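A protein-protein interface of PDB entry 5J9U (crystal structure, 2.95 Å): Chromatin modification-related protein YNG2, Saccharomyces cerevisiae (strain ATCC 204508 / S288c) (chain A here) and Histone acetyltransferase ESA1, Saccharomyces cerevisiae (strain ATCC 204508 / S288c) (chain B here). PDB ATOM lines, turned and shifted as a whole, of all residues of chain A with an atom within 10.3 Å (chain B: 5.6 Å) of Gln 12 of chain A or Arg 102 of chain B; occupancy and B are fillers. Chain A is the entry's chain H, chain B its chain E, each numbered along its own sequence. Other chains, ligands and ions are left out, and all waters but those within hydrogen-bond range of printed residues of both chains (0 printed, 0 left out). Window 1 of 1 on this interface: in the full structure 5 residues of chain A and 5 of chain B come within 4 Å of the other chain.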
ATOM      1  N   SER A   4     -16.349   6.443  17.732  1.00  0.00           N
ATOM      2  CA  SER A   4     -15.132   7.244  17.762  1.00  0.00           C
ATOM      3  C   SER A   4     -14.434   7.237  16.411  1.00  0.00           C
ATOM      4  O   SER A   4     -13.730   8.194  16.069  1.00  0.00           O
ATOM      5  CB  SER A   4     -14.193   6.724  18.851  1.00  0.00           C
ATOM      6  OG  SER A   4     -13.651   5.465  18.491  1.00  0.00           O
ATOM      7  N   LEU A   5     -14.617   6.170  15.636  1.00  0.00           N
ATOM      8  CA  LEU A   5     -14.037   6.098  14.302  1.00  0.00           C
ATOM      9  C   LEU A   5     -14.828   6.945  13.313  1.00  0.00           C
ATOM     10  O   LEU A   5     -14.241   7.620  12.460  1.00  0.00           O
ATOM     11  CB  LEU A   5     -13.975   4.641  13.847  1.00  0.00           C
ATOM     12  CG  LEU A   5     -13.409   4.314  12.466  1.00  0.00           C
ATOM     13  CD1 LEU A   5     -12.011   4.884  12.306  1.00  0.00           C
ATOM     14  CD2 LEU A   5     -13.407   2.810  12.265  1.00  0.00           C
ATOM     15  N   VAL A   6     -16.158   6.920  13.416  1.00  0.00           N
ATOM     16  CA  VAL A   6     -16.993   7.757  12.560  1.00  0.00           C
ATOM     17  C   VAL A   6     -16.813   9.228  12.911  1.00  0.00           C
ATOM     18  O   VAL A   6     -16.786  10.093  12.027  1.00  0.00           O
ATOM     19  CB  VAL A   6     -18.467   7.325  12.669  1.00  0.00           C
ATOM     20  CG1 VAL A   6     -19.350   8.252  11.860  1.00  0.00           C
ATOM     21  CG2 VAL A   6     -18.631   5.886  12.208  1.00  0.00           C
ATOM     22  N   LEU A   7     -16.689   9.537  14.204  1.00  0.00           N
ATOM     23  CA  LEU A   7     -16.451  10.915  14.620  1.00  0.00           C
ATOM     24  C   LEU A   7     -15.125  11.433  14.081  1.00  0.00           C
ATOM     25  O   LEU A   7     -15.060  12.523  13.502  1.00  0.00           O
ATOM     26  CB  LEU A   7     -16.476  11.020  16.142  1.00  0.00           C
ATOM     27  CG  LEU A   7     -16.104  12.409  16.656  1.00  0.00           C
ATOM     28  CD1 LEU A   7     -17.127  13.453  16.237  1.00  0.00           C
ATOM     29  CD2 LEU A   7     -15.941  12.379  18.152  1.00  0.00           C
ATOM     30  N   GLU A   8     -14.050  10.667  14.284  1.00  0.00           N
ATOM     31  CA  GLU A   8     -12.752  11.038  13.728  1.00  0.00           C
ATOM     32  C   GLU A   8     -12.845  11.257  12.225  1.00  0.00           C
ATOM     33  O   GLU A   8     -12.268  12.210  11.689  1.00  0.00           O
ATOM     34  CB  GLU A   8     -11.720   9.959  14.053  1.00  0.00           C
ATOM     35  CG  GLU A   8     -10.415  10.095  13.291  1.00  0.00           C
ATOM     36  CD  GLU A   8      -9.662   8.783  13.191  1.00  0.00           C
ATOM     37  OE1 GLU A   8      -9.844   7.923  14.078  1.00  0.00           O
ATOM     38  OE2 GLU A   8      -8.890   8.612  12.224  1.00  0.00           O
ATOM     39  N   GLN A   9     -13.578  10.385  11.530  1.00  0.00           N
ATOM     40  CA  GLN A   9     -13.676  10.489  10.079  1.00  0.00           C
ATOM     41  C   GLN A   9     -14.506  11.699   9.671  1.00  0.00           C
ATOM     42  O   GLN A   9     -14.147  12.416   8.729  1.00  0.00           O
ATOM     43  CB  GLN A   9     -14.275   9.207   9.504  1.00  0.00           C
ATOM     44  CG  GLN A   9     -14.093   9.056   8.006  1.00  0.00           C
ATOM     45  CD  GLN A   9     -12.633   9.070   7.601  1.00  0.00           C
ATOM     46  OE1 GLN A   9     -12.168  10.000   6.943  1.00  0.00           O
ATOM     47  NE2 GLN A   9     -11.900   8.035   7.997  1.00  0.00           N
ATOM     48  N   THR A  10     -15.619  11.942  10.369  1.00  0.00           N
ATOM     49  CA  THR A  10     -16.479  13.068  10.023  1.00  0.00           C
ATOM     50  C   THR A  10     -15.800  14.396  10.337  1.00  0.00           C
ATOM     51  O   THR A  10     -15.952  15.368   9.587  1.00  0.00           O
ATOM     52  CB  THR A  10     -17.816  12.958  10.762  1.00  0.00           C
ATOM     53  OG1 THR A  10     -18.488  11.753  10.367  1.00  0.00           O
ATOM     54  CG2 THR A  10     -18.710  14.151  10.445  1.00  0.00           C
ATOM     55  N   ILE A  11     -15.036  14.451  11.431  1.00  0.00           N
ATOM     56  CA  ILE A  11     -14.332  15.680  11.799  1.00  0.00           C
ATOM     57  C   ILE A  11     -13.359  16.083  10.699  1.00  0.00           C
ATOM     58  O   ILE A  11     -13.301  17.249  10.289  1.00  0.00           O
ATOM     59  CB  ILE A  11     -13.607  15.502  13.145  1.00  0.00           C
ATOM     60  CG1 ILE A  11     -14.596  15.578  14.308  1.00  0.00           C
ATOM     61  CG2 ILE A  11     -12.505  16.544  13.304  1.00  0.00           C
ATOM     62  CD1 ILE A  11     -13.944  15.418  15.664  1.00  0.00           C
ATOM     63  N   GLN A  12     -12.586  15.117  10.201  1.00  0.00           N
ATOM     64  CA  GLN A  12     -11.616  15.404   9.150  1.00  0.00           C
ATOM     65  C   GLN A  12     -12.304  15.802   7.849  1.00  0.00           C
ATOM     66  O   GLN A  12     -11.832  16.702   7.143  1.00  0.00           O
ATOM     67  CB  GLN A  12     -10.708  14.190   8.944  1.00  0.00           C
ATOM     68  CG  GLN A  12      -9.755  14.302   7.770  1.00  0.00           C
ATOM     69  CD  GLN A  12      -8.867  13.083   7.632  1.00  0.00           C
ATOM     70  OE1 GLN A  12      -8.830  12.224   8.513  1.00  0.00           O
ATOM     71  NE2 GLN A  12      -8.145  13.000   6.522  1.00  0.00           N
ATOM     72  N   ASP A  13     -13.425  15.156   7.522  1.00  0.00           N
ATOM     73  CA  ASP A  13     -14.100  15.419   6.254  1.00  0.00           C
ATOM     74  C   ASP A  13     -14.724  16.810   6.189  1.00  0.00           C
ATOM     75  O   ASP A  13     -14.916  17.334   5.086  1.00  0.00           O
ATOM     76  CB  ASP A  13     -15.164  14.350   6.001  1.00  0.00           C
ATOM     77  CG  ASP A  13     -14.586  13.087   5.388  1.00  0.00           C
ATOM     78  OD1 ASP A  13     -13.358  12.882   5.495  1.00  0.00           O
ATOM     79  OD2 ASP A  13     -15.358  12.299   4.800  1.00  0.00           O
ATOM     80  N   VAL A  14     -15.051  17.413   7.330  1.00  0.00           N
ATOM     81  CA  VAL A  14     -15.676  18.731   7.374  1.00  0.00           C
ATOM     82  C   VAL A  14     -14.724  19.794   7.911  1.00  0.00           C
ATOM     83  O   VAL A  14     -15.156  20.914   8.205  1.00  0.00           O
ATOM     84  CB  VAL A  14     -16.977  18.707   8.196  1.00  0.00           C
ATOM     85  CG1 VAL A  14     -17.948  17.673   7.640  1.00  0.00           C
ATOM     86  CG2 VAL A  14     -16.683  18.446   9.666  1.00  0.00           C
ATOM     87  N   SER A  15     -13.435  19.470   8.047  1.00  0.00           N
ATOM     88  CA  SER A  15     -12.500  20.370   8.718  1.00  0.00           C
ATOM     89  C   SER A  15     -12.339  21.694   7.977  1.00  0.00           C
ATOM     90  O   SER A  15     -12.255  22.756   8.607  1.00  0.00           O
ATOM     91  CB  SER A  15     -11.145  19.684   8.879  1.00  0.00           C
ATOM     92  OG  SER A  15     -10.607  19.321   7.619  1.00  0.00           O
ATOM     93  N   ASN A  16     -12.300  21.661   6.647  1.00  0.00           N
ATOM     94  CA  ASN A  16     -12.064  22.863   5.857  1.00  0.00           C
ATOM     95  C   ASN A  16     -13.361  23.497   5.374  1.00  0.00           C
ATOM     96  O   ASN A  16     -13.324  24.501   4.654  1.00  0.00           O
ATOM     97  CB  ASN A  16     -11.146  22.539   4.667  1.00  0.00           C
ATOM     98  CG  ASN A  16     -10.676  23.785   3.927  1.00  0.00           C
ATOM     99  OD1 ASN A  16      -9.951  24.613   4.480  1.00  0.00           O
ATOM    100  ND2 ASN A  16     -11.080  23.915   2.667  1.00  0.00           N
ATOM    101  N   LEU A  17     -14.506  22.944   5.769  1.00  0.00           N
ATOM    102  CA  LEU A  17     -15.816  23.439   5.363  1.00  0.00           C
ATOM    103  C   LEU A  17     -16.116  24.833   5.912  1.00  0.00           C
ATOM    104  O   LEU A  17     -16.627  25.675   5.161  1.00  0.00           O
ATOM    105  CB  LEU A  17     -16.910  22.459   5.793  1.00  0.00           C
ATOM    106  CG  LEU A  17     -18.272  22.724   5.152  1.00  0.00           C
ATOM    107  CD1 LEU A  17     -18.164  22.644   3.636  1.00  0.00           C
ATOM    108  CD2 LEU A  17     -19.311  21.750   5.674  1.00  0.00           C
ATOM    109  N   PRO A  18     -15.836  25.129   7.192  1.00  0.00           N
ATOM    110  CA  PRO A  18     -16.064  26.507   7.659  1.00  0.00           C
ATOM    111  C   PRO A  18     -15.232  27.531   6.908  1.00  0.00           C
ATOM    112  O   PRO A  18     -15.708  28.642   6.650  1.00  0.00           O
ATOM    113  CB  PRO A  18     -15.691  26.441   9.148  1.00  0.00           C
ATOM    114  CG  PRO A  18     -14.856  25.228   9.285  1.00  0.00           C
ATOM    115  CD  PRO A  18     -15.416  24.259   8.304  1.00  0.00           C
ATOM    116  N   GLU A  20     -14.369  27.136   3.811  1.00  0.00           N
ATOM    117  CA  GLU A  20     -14.955  27.176   2.476  1.00  0.00           C
ATOM    118  C   GLU A  20     -16.208  28.039   2.448  1.00  0.00           C
ATOM    119  O   GLU A  20     -16.450  28.759   1.473  1.00  0.00           O
ATOM    120  CB  GLU A  20     -15.285  25.759   2.012  1.00  0.00           C
ATOM    121  CG  GLU A  20     -14.184  25.080   1.236  1.00  0.00           C
ATOM    122  CD  GLU A  20     -14.360  23.578   1.188  1.00  0.00           C
ATOM    123  OE1 GLU A  20     -15.182  23.046   1.965  1.00  0.00           O
ATOM    124  OE2 GLU A  20     -13.692  22.934   0.357  1.00  0.00           O
ATOM    125  N   HIS A 100     -21.984  16.080   3.130  1.00  0.00           N
ATOM    126  CA  HIS A 100     -21.385  15.613   4.376  1.00  0.00           C
ATOM    127  C   HIS A 100     -22.459  15.195   5.369  1.00  0.00           C
ATOM    128  O   HIS A 100     -22.300  14.204   6.091  1.00  0.00           O
ATOM    129  CB  HIS A 100     -20.508  16.705   4.991  1.00  0.00           C
ATOM    130  CG  HIS A 100     -19.275  17.007   4.201  1.00  0.00           C
ATOM    131  ND1 HIS A 100     -18.571  18.183   4.345  1.00  0.00           N
ATOM    132  CD2 HIS A 100     -18.622  16.289   3.258  1.00  0.00           C
ATOM    133  CE1 HIS A 100     -17.537  18.176   3.524  1.00  0.00           C
ATOM    134  NE2 HIS A 100     -17.544  17.038   2.854  1.00  0.00           N
ATOM    135  N   LYS A 103     -23.719  11.755   4.357  1.00  0.00           N
ATOM    136  CA  LYS A 103     -22.772  10.698   4.702  1.00  0.00           C
ATOM    137  C   LYS A 103     -22.783  10.408   6.199  1.00  0.00           C
ATOM    138  O   LYS A 103     -22.793   9.243   6.612  1.00  0.00           O
ATOM    139  CB  LYS A 103     -21.365  11.067   4.235  1.00  0.00           C
ATOM    140  CG  LYS A 103     -20.351   9.953   4.456  1.00  0.00           C
ATOM    141  CD  LYS A 103     -19.018  10.265   3.798  1.00  0.00           C
ATOM    142  CE  LYS A 103     -17.887  10.272   4.816  1.00  0.00           C
ATOM    143  NZ  LYS A 103     -17.756   8.971   5.530  1.00  0.00           N
ATOM    144  N   LEU A 104     -22.778  11.455   7.027  1.00  0.00           N
ATOM    145  CA  LEU A 104     -22.848  11.257   8.472  1.00  0.00           C
ATOM    146  C   LEU A 104     -24.138  10.556   8.868  1.00  0.00           C
ATOM    147  O   LEU A 104     -24.133   9.659   9.720  1.00  0.00           O
ATOM    148  CB  LEU A 104     -22.737  12.601   9.192  1.00  0.00           C
ATOM    149  CG  LEU A 104     -23.021  12.592  10.697  1.00  0.00           C
ATOM    150  CD1 LEU A 104     -22.066  11.667  11.433  1.00  0.00           C
ATOM    151  CD2 LEU A 104     -22.957  14.000  11.261  1.00  0.00           C
ATOM    152  N   ASP B 100      -3.384  17.685   1.791  1.00  0.00           N
ATOM    153  CA  ASP B 100      -3.250  16.539   2.680  1.00  0.00           C
ATOM    154  C   ASP B 100      -3.385  15.252   1.874  1.00  0.00           C
ATOM    155  O   ASP B 100      -4.368  15.066   1.150  1.00  0.00           O
ATOM    156  CB  ASP B 100      -4.315  16.596   3.778  1.00  0.00           C
ATOM    157  CG  ASP B 100      -4.069  15.598   4.900  1.00  0.00           C
ATOM    158  OD1 ASP B 100      -4.406  15.922   6.059  1.00  0.00           O
ATOM    159  OD2 ASP B 100      -3.547  14.494   4.638  1.00  0.00           O
ATOM    160  N   GLY B 101      -2.397  14.363   2.006  1.00  0.00           N
ATOM    161  CA  GLY B 101      -2.451  13.090   1.308  1.00  0.00           C
ATOM    162  C   GLY B 101      -3.579  12.186   1.754  1.00  0.00           C
ATOM    163  O   GLY B 101      -4.004  11.316   0.986  1.00  0.00           O
ATOM    164  N   ARG B 102      -4.080  12.374   2.976  1.00  0.00           N
ATOM    165  CA  ARG B 102      -5.175  11.544   3.465  1.00  0.00           C
ATOM    166  C   ARG B 102      -6.524  12.032   2.950  1.00  0.00           C
ATOM    167  O   ARG B 102      -7.460  11.234   2.826  1.00  0.00           O
ATOM    168  CB  ARG B 102      -5.156  11.503   4.996  1.00  0.00           C
ATOM    169  CG  ARG B 102      -6.122  10.502   5.618  1.00  0.00           C
ATOM    170  CD  ARG B 102      -5.887  10.356   7.116  1.00  0.00           C
ATOM    171  NE  ARG B 102      -7.026   9.740   7.790  1.00  0.00           N
ATOM    172  CZ  ARG B 102      -7.046   9.411   9.078  1.00  0.00           C
ATOM    173  NH1 ARG B 102      -5.983   9.633   9.840  1.00  0.00           N
ATOM    174  NH2 ARG B 102      -8.128   8.855   9.604  1.00  0.00           N
ATOM    175  N   LYS B 103      -6.638  13.322   2.637  1.00  0.00           N
ATOM    176  CA  LYS B 103      -7.867  13.884   2.088  1.00  0.00           C
ATOM    177  C   LYS B 103      -7.923  13.793   0.568  1.00  0.00           C
ATOM    178  O   LYS B 103      -8.989  13.526   0.003  1.00  0.00           O
ATOM    179  CB  LYS B 103      -8.025  15.345   2.516  1.00  0.00           C
ATOM    180  CG  LYS B 103      -8.291  15.547   3.994  1.00  0.00           C
ATOM    181  CD  LYS B 103      -8.768  16.966   4.256  1.00  0.00           C
ATOM    182  CE  LYS B 103      -9.041  17.198   5.730  1.00  0.00           C
ATOM    183  NZ  LYS B 103      -7.837  16.973   6.576  1.00  0.00           N
ATOM    184  N   GLN B 104      -6.799  14.007  -0.106  1.00  0.00           N
ATOM    185  CA  GLN B 104      -6.745  13.987  -1.561  1.00  0.00           C
ATOM    186  C   GLN B 104      -5.926  12.776  -1.998  1.00  0.00           C
ATOM    187  O   GLN B 104      -4.826  12.896  -2.541  1.00  0.00           O
ATOM    188  CB  GLN B 104      -6.143  15.293  -2.083  1.00  0.00           C
ATOM    189  CG  GLN B 104      -6.877  16.546  -1.625  1.00  0.00           C
ATOM    190  CD  GLN B 104      -8.278  16.652  -2.180  1.00  0.00           C
ATOM    191  OE1 GLN B 104      -8.595  16.072  -3.219  1.00  0.00           O
ATOM    192  NE2 GLN B 104      -9.132  17.395  -1.486  1.00  0.00           N
ATOM    193  N   ARG B 105      -6.491  11.590  -1.757  1.00  0.00           N
ATOM    194  CA  ARG B 105      -5.761  10.348  -2.002  1.00  0.00           C
ATOM    195  C   ARG B 105      -5.431  10.172  -3.480  1.00  0.00           C
ATOM    196  O   ARG B 105      -4.269   9.965  -3.846  1.00  0.00           O
ATOM    197  CB  ARG B 105      -6.561   9.156  -1.474  1.00  0.00           C
ATOM    198  CG  ARG B 105      -5.912   7.811  -1.764  1.00  0.00           C
ATOM    199  CD  ARG B 105      -6.409   6.703  -0.843  1.00  0.00           C
ATOM    200  NE  ARG B 105      -6.016   6.911   0.548  1.00  0.00           N
ATOM    201  CZ  ARG B 105      -6.847   7.272   1.521  1.00  0.00           C
ATOM    202  NH1 ARG B 105      -6.392   7.434   2.756  1.00  0.00           N
ATOM    203  NH2 ARG B 105      -8.133   7.463   1.263  1.00  0.00           N
ATOM    204  N   VAL B 128      -0.221   7.418   0.463  1.00  0.00           N
ATOM    205  CA  VAL B 128       0.156   8.823   0.614  1.00  0.00           C
ATOM    206  C   VAL B 128      -0.386   9.452   1.884  1.00  0.00           C
ATOM    207  O   VAL B 128      -0.205  10.661   2.087  1.00  0.00           O
ATOM    208  CB  VAL B 128      -0.321   9.646  -0.599  1.00  0.00           C
ATOM    209  CG1 VAL B 128       0.455   9.241  -1.837  1.00  0.00           C
ATOM    210  CG2 VAL B 128      -1.812   9.450  -0.814  1.00  0.00           C
ATOM    211  N   ASP B 129      -1.059   8.675   2.736  1.00  0.00           N
ATOM    212  CA  ASP B 129      -1.645   9.200   3.970  1.00  0.00           C
ATOM    213  C   ASP B 129      -0.689  10.010   4.842  1.00  0.00           C
ATOM    214  O   ASP B 129      -1.087  11.093   5.298  1.00  0.00           O
ATOM    215  CB  ASP B 129      -2.249   8.046   4.787  1.00  0.00           C
ATOM    216  CG  ASP B 129      -3.519   7.489   4.171  1.00  0.00           C
ATOM    217  OD1 ASP B 129      -4.092   8.157   3.284  1.00  0.00           O
ATOM    218  OD2 ASP B 129      -3.961   6.401   4.595  1.00  0.00           O
ATOM    219  N   PHE B 131       1.643  12.089   4.436  1.00  0.00           N
ATOM    220  CA  PHE B 131       2.351  13.225   3.865  1.00  0.00           C
ATOM    221  C   PHE B 131       1.476  14.458   3.684  1.00  0.00           C
ATOM    222  O   PHE B 131       0.270  14.370   3.445  1.00  0.00           O
ATOM    223  CB  PHE B 131       2.974  12.859   2.519  1.00  0.00           C
ATOM    224  CG  PHE B 131       4.119  11.908   2.629  1.00  0.00           C
ATOM    225  CD1 PHE B 131       3.958  10.567   2.333  1.00  0.00           C
ATOM    226  CD2 PHE B 131       5.359  12.354   3.053  1.00  0.00           C
ATOM    227  CE1 PHE B 131       5.015   9.692   2.440  1.00  0.00           C
ATOM    228  CE2 PHE B 131       6.420  11.486   3.162  1.00  0.00           C
ATOM    229  CZ  PHE B 131       6.249  10.152   2.856  1.00  0.00           C
ATOM    230  N   LYS B 154       4.010  14.576   8.120  1.00  0.00           N
ATOM    231  CA  LYS B 154       3.036  15.373   8.863  1.00  0.00           C
ATOM    232  C   LYS B 154       3.627  15.896  10.166  1.00  0.00           C
ATOM    233  O   LYS B 154       3.486  17.080  10.495  1.00  0.00           O
ATOM    234  CB  LYS B 154       1.777  14.547   9.124  1.00  0.00           C
ATOM    235  CG  LYS B 154       0.838  14.465   7.928  1.00  0.00           C
ATOM    236  CD  LYS B 154      -0.512  13.886   8.315  1.00  0.00           C
ATOM    237  CE  LYS B 154      -1.504  13.971   7.166  1.00  0.00           C
ATOM    238  NZ  LYS B 154      -2.836  13.423   7.547  1.00  0.00           N
ATOM    239  N   SER B 299      -5.352  10.448  16.537  1.00  0.00           N
ATOM    240  CA  SER B 299      -6.102   9.625  15.596  1.00  0.00           C
ATOM    241  C   SER B 299      -5.886  10.081  14.159  1.00  0.00           C
ATOM    242  O   SER B 299      -5.949   9.263  13.233  1.00  0.00           O
ATOM    243  CB  SER B 299      -7.590   9.654  15.942  1.00  0.00           C
ATOM    244  OG  SER B 299      -8.110  10.969  15.854  1.00  0.00           O
ATOM    245  N   GLN B 300      -5.632  11.374  13.951  1.00  0.00           N
ATOM    246  CA  GLN B 300      -5.356  11.878  12.611  1.00  0.00           C
ATOM    247  C   GLN B 300      -3.976  11.468  12.113  1.00  0.00           C
ATOM    248  O   GLN B 300      -3.748  11.455  10.898  1.00  0.00           O
ATOM    249  CB  GLN B 300      -5.503  13.399  12.588  1.00  0.00           C
ATOM    250  CG  GLN B 300      -6.907  13.875  12.924  1.00  0.00           C
ATOM    251  CD  GLN B 300      -7.016  15.384  12.989  1.00  0.00           C
ATOM    252  OE1 GLN B 300      -6.044  16.075  13.288  1.00  0.00           O
ATOM    253  NE2 GLN B 300      -8.208  15.903  12.720  1.00  0.00           N
ATOM    254  N   LEU B 301      -3.055  11.136  13.014  1.00  0.00           N
ATOM    255  CA  LEU B 301      -1.722  10.673  12.625  1.00  0.00           C
ATOM    256  C   LEU B 301      -1.693   9.160  12.451  1.00  0.00           C
ATOM    257  O   LEU B 301      -0.830   8.460  12.978  1.00  0.00           O
ATOM    258  CB  LEU B 301      -0.686  11.128  13.646  1.00  0.00           C
ATOM    259  CG  LEU B 301      -0.356  12.619  13.637  1.00  0.00           C
ATOM    260  CD1 LEU B 301       0.778  12.920  14.603  1.00  0.00           C
ATOM    261  CD2 LEU B 301      -0.005  13.075  12.231  1.00  0.00           C
ATOM    262  N   ARG B 302      -2.668   8.649  11.704  1.00  0.00           N
ATOM    263  CA  ARG B 302      -2.759   7.234  11.384  1.00  0.00           C
ATOM    264  C   ARG B 302      -3.178   7.106   9.927  1.00  0.00           C
ATOM    265  O   ARG B 302      -3.515   8.093   9.268  1.00  0.00           O
ATOM    266  CB  ARG B 302      -3.760   6.510  12.297  1.00  0.00           C
ATOM    267  CG  ARG B 302      -3.538   6.732  13.786  1.00  0.00           C
ATOM    268  CD  ARG B 302      -4.427   5.825  14.617  1.00  0.00           C
ATOM    269  NE  ARG B 302      -4.108   4.418  14.398  1.00  0.00           N
ATOM    270  CZ  ARG B 302      -4.550   3.423  15.157  1.00  0.00           C
ATOM    271  NH1 ARG B 302      -5.337   3.672  16.196  1.00  0.00           N
ATOM    272  NH2 ARG B 302      -4.203   2.174  14.877  1.00  0.00           N
ATOM    273  N   PHE B 303      -3.155   5.879   9.421  1.00  0.00           N
ATOM    274  CA  PHE B 303      -3.730   5.621   8.112  1.00  0.00           C
ATOM    275  C   PHE B 303      -5.245   5.513   8.243  1.00  0.00           C
ATOM    276  O   PHE B 303      -5.768   5.037   9.254  1.00  0.00           O
ATOM    277  CB  PHE B 303      -3.148   4.344   7.503  1.00  0.00           C
ATOM    278  CG  PHE B 303      -1.762   4.516   6.934  1.00  0.00           C
ATOM    279  CD1 PHE B 303      -1.563   4.569   5.565  1.00  0.00           C
ATOM    280  CD2 PHE B 303      -0.662   4.629   7.769  1.00  0.00           C
ATOM    281  CE1 PHE B 303      -0.292   4.729   5.039  1.00  0.00           C
ATOM    282  CE2 PHE B 303       0.611   4.788   7.251  1.00  0.00           C
ATOM    283  CZ  PHE B 303       0.796   4.838   5.884  1.00  0.00           C
ATOM    284  N   ALA B 304      -5.948   5.964   7.209  1.00  0.00           N
ATOM    285  CA  ALA B 304      -7.402   6.004   7.256  1.00  0.00           C
ATOM    286  C   ALA B 304      -7.989   4.598   7.325  1.00  0.00           C
ATOM    287  O   ALA B 304      -7.414   3.632   6.818  1.00  0.00           O
ATOM    288  CB  ALA B 304      -7.957   6.746   6.040  1.00  0.00           C
ATOM    289  N   TRP B 305      -9.151   4.494   7.963  1.00  0.00           N
ATOM    290  CA  TRP B 305      -9.822   3.213   8.145  1.00  0.00           C
ATOM    291  C   TRP B 305     -11.305   3.331   7.808  1.00  0.00           C
ATOM    292  O   TRP B 305     -11.911   2.393   7.290  1.00  0.00           O
ATOM    293  CB  TRP B 305      -9.645   2.714   9.581  1.00  0.00           C
ATOM    294  CG  TRP B 305     -10.110   1.302   9.806  1.00  0.00           C
ATOM    295  CD1 TRP B 305     -11.266   0.909  10.415  1.00  0.00           C
ATOM    296  CD2 TRP B 305      -9.420   0.098   9.442  1.00  0.00           C
ATOM    297  NE1 TRP B 305     -11.345  -0.462  10.446  1.00  0.00           N
ATOM    298  CE2 TRP B 305     -10.223  -0.984   9.855  1.00  0.00           C
ATOM    299  CE3 TRP B 305      -8.206  -0.168   8.804  1.00  0.00           C
ATOM    300  CZ2 TRP B 305      -9.851  -2.312   9.650  1.00  0.00           C
ATOM    301  CZ3 TRP B 305      -7.837  -1.488   8.602  1.00  0.00           C
ATOM    302  CH2 TRP B 305      -8.658  -2.542   9.024  1.00  0.00           C
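The side-chain carboxylate (OE2) of Glu 8 of chain A is in salt-bridge range of the guanidinium group (NH2) of Arg 102 of chain B (2.7 Å).
NE of Arg 102 of chain B sits at hydrogen-bond distance from OE1 of Gln 12 of chain A (3.2 Å).
O of Ser 299 of chain B sits close to OE2 of Glu 8 of chain A.
The backbone NH (N) of Arg 102 of chain B is in hydrogen-bond range of the side-chain carboxylate (OD2) of Asp 100 of chain B, at 2.7 Å.
The side-chain carboxylate (OD1) of Asp 100 of chain B is in salt-bridge range of the side-chain amino group (NZ) of Lys 103 of chain B (3.6 Å).
The backbone carbonyl oxygen (O) of Ser 299 of chain B sits at hydrogen-bond distance from the guanidinium group (NH1) of Arg 102 of chain B.
The guanidinium group (NH1) of Arg 102 of chain B lies within hydrogen-bond range of the backbone carbonyl oxygen (O) of Gln 300 of chain B.
The guanidinium group (NH1) of Arg 102 of chain B is in hydrogen-bond range of the backbone carbonyl oxygen (O) of Arg 302 of chain B, 3.0 Å away.
The backbone carbonyl oxygen of Gln 12 of chain A is in hydrogen-bond range of the side-chain hydroxyl of Ser 15 of chain A, 2.9 Å away.
CD2 of Leu 5 of chain A touches CD1 of Trp 305 of chain B, 3.4 Å away.
CE of Lys 103 of chain B touches O of Gln 12 of chain A (3.2 Å).
OG of Ser 15 of chain A touches CE of Lys 103 of chain B, 3.2 Å away.
Of the printed residues of chain B, Leu 5 of chain A touches Trp 305 (3.4 Å).
Gln 12 of chain A touches just these residues of chain B: Arg 102 (3.2 Å) and Lys 103 (3.2 Å).
Printed residues of chain B within 4 Å of Ser 15 of chain A: Lys 103.
No residue of chain A comes within 4 Å of Asp 100 of chain B.
No residue of chain A comes within 4 Å of Gly 101 of chain B.
Arg 102 of chain B touches two residues of chain A.
Lys 103 of chain B touches just these residues of chain A: Gln 12 (3.2 Å) and Ser 15 (3.2 Å).
No residue of chain A comes within 4 Å of Ala 304 of chain B.
Of the printed residues of chain A, Trp 305 of chain B touches Leu 5 (3.4 Å).
Printed residues of chain B that touch a printed residue of chain A: Arg 102, Lys 103, Ser 299 and Trp 305.
Hydrophobic or aromatic side chains of chain B within 4 Å of the printed part of chain A: Trp 305.
Printed residues of chain A that touch a printed residue of chain B: Leu 5, Glu 8, Gln 12 and Ser 15.
Hydrophobic or aromatic side chains of chain A within 4 Å of the printed part of chain B: Leu 5.
Among the printed residues, 6 pairs touch across the chains.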
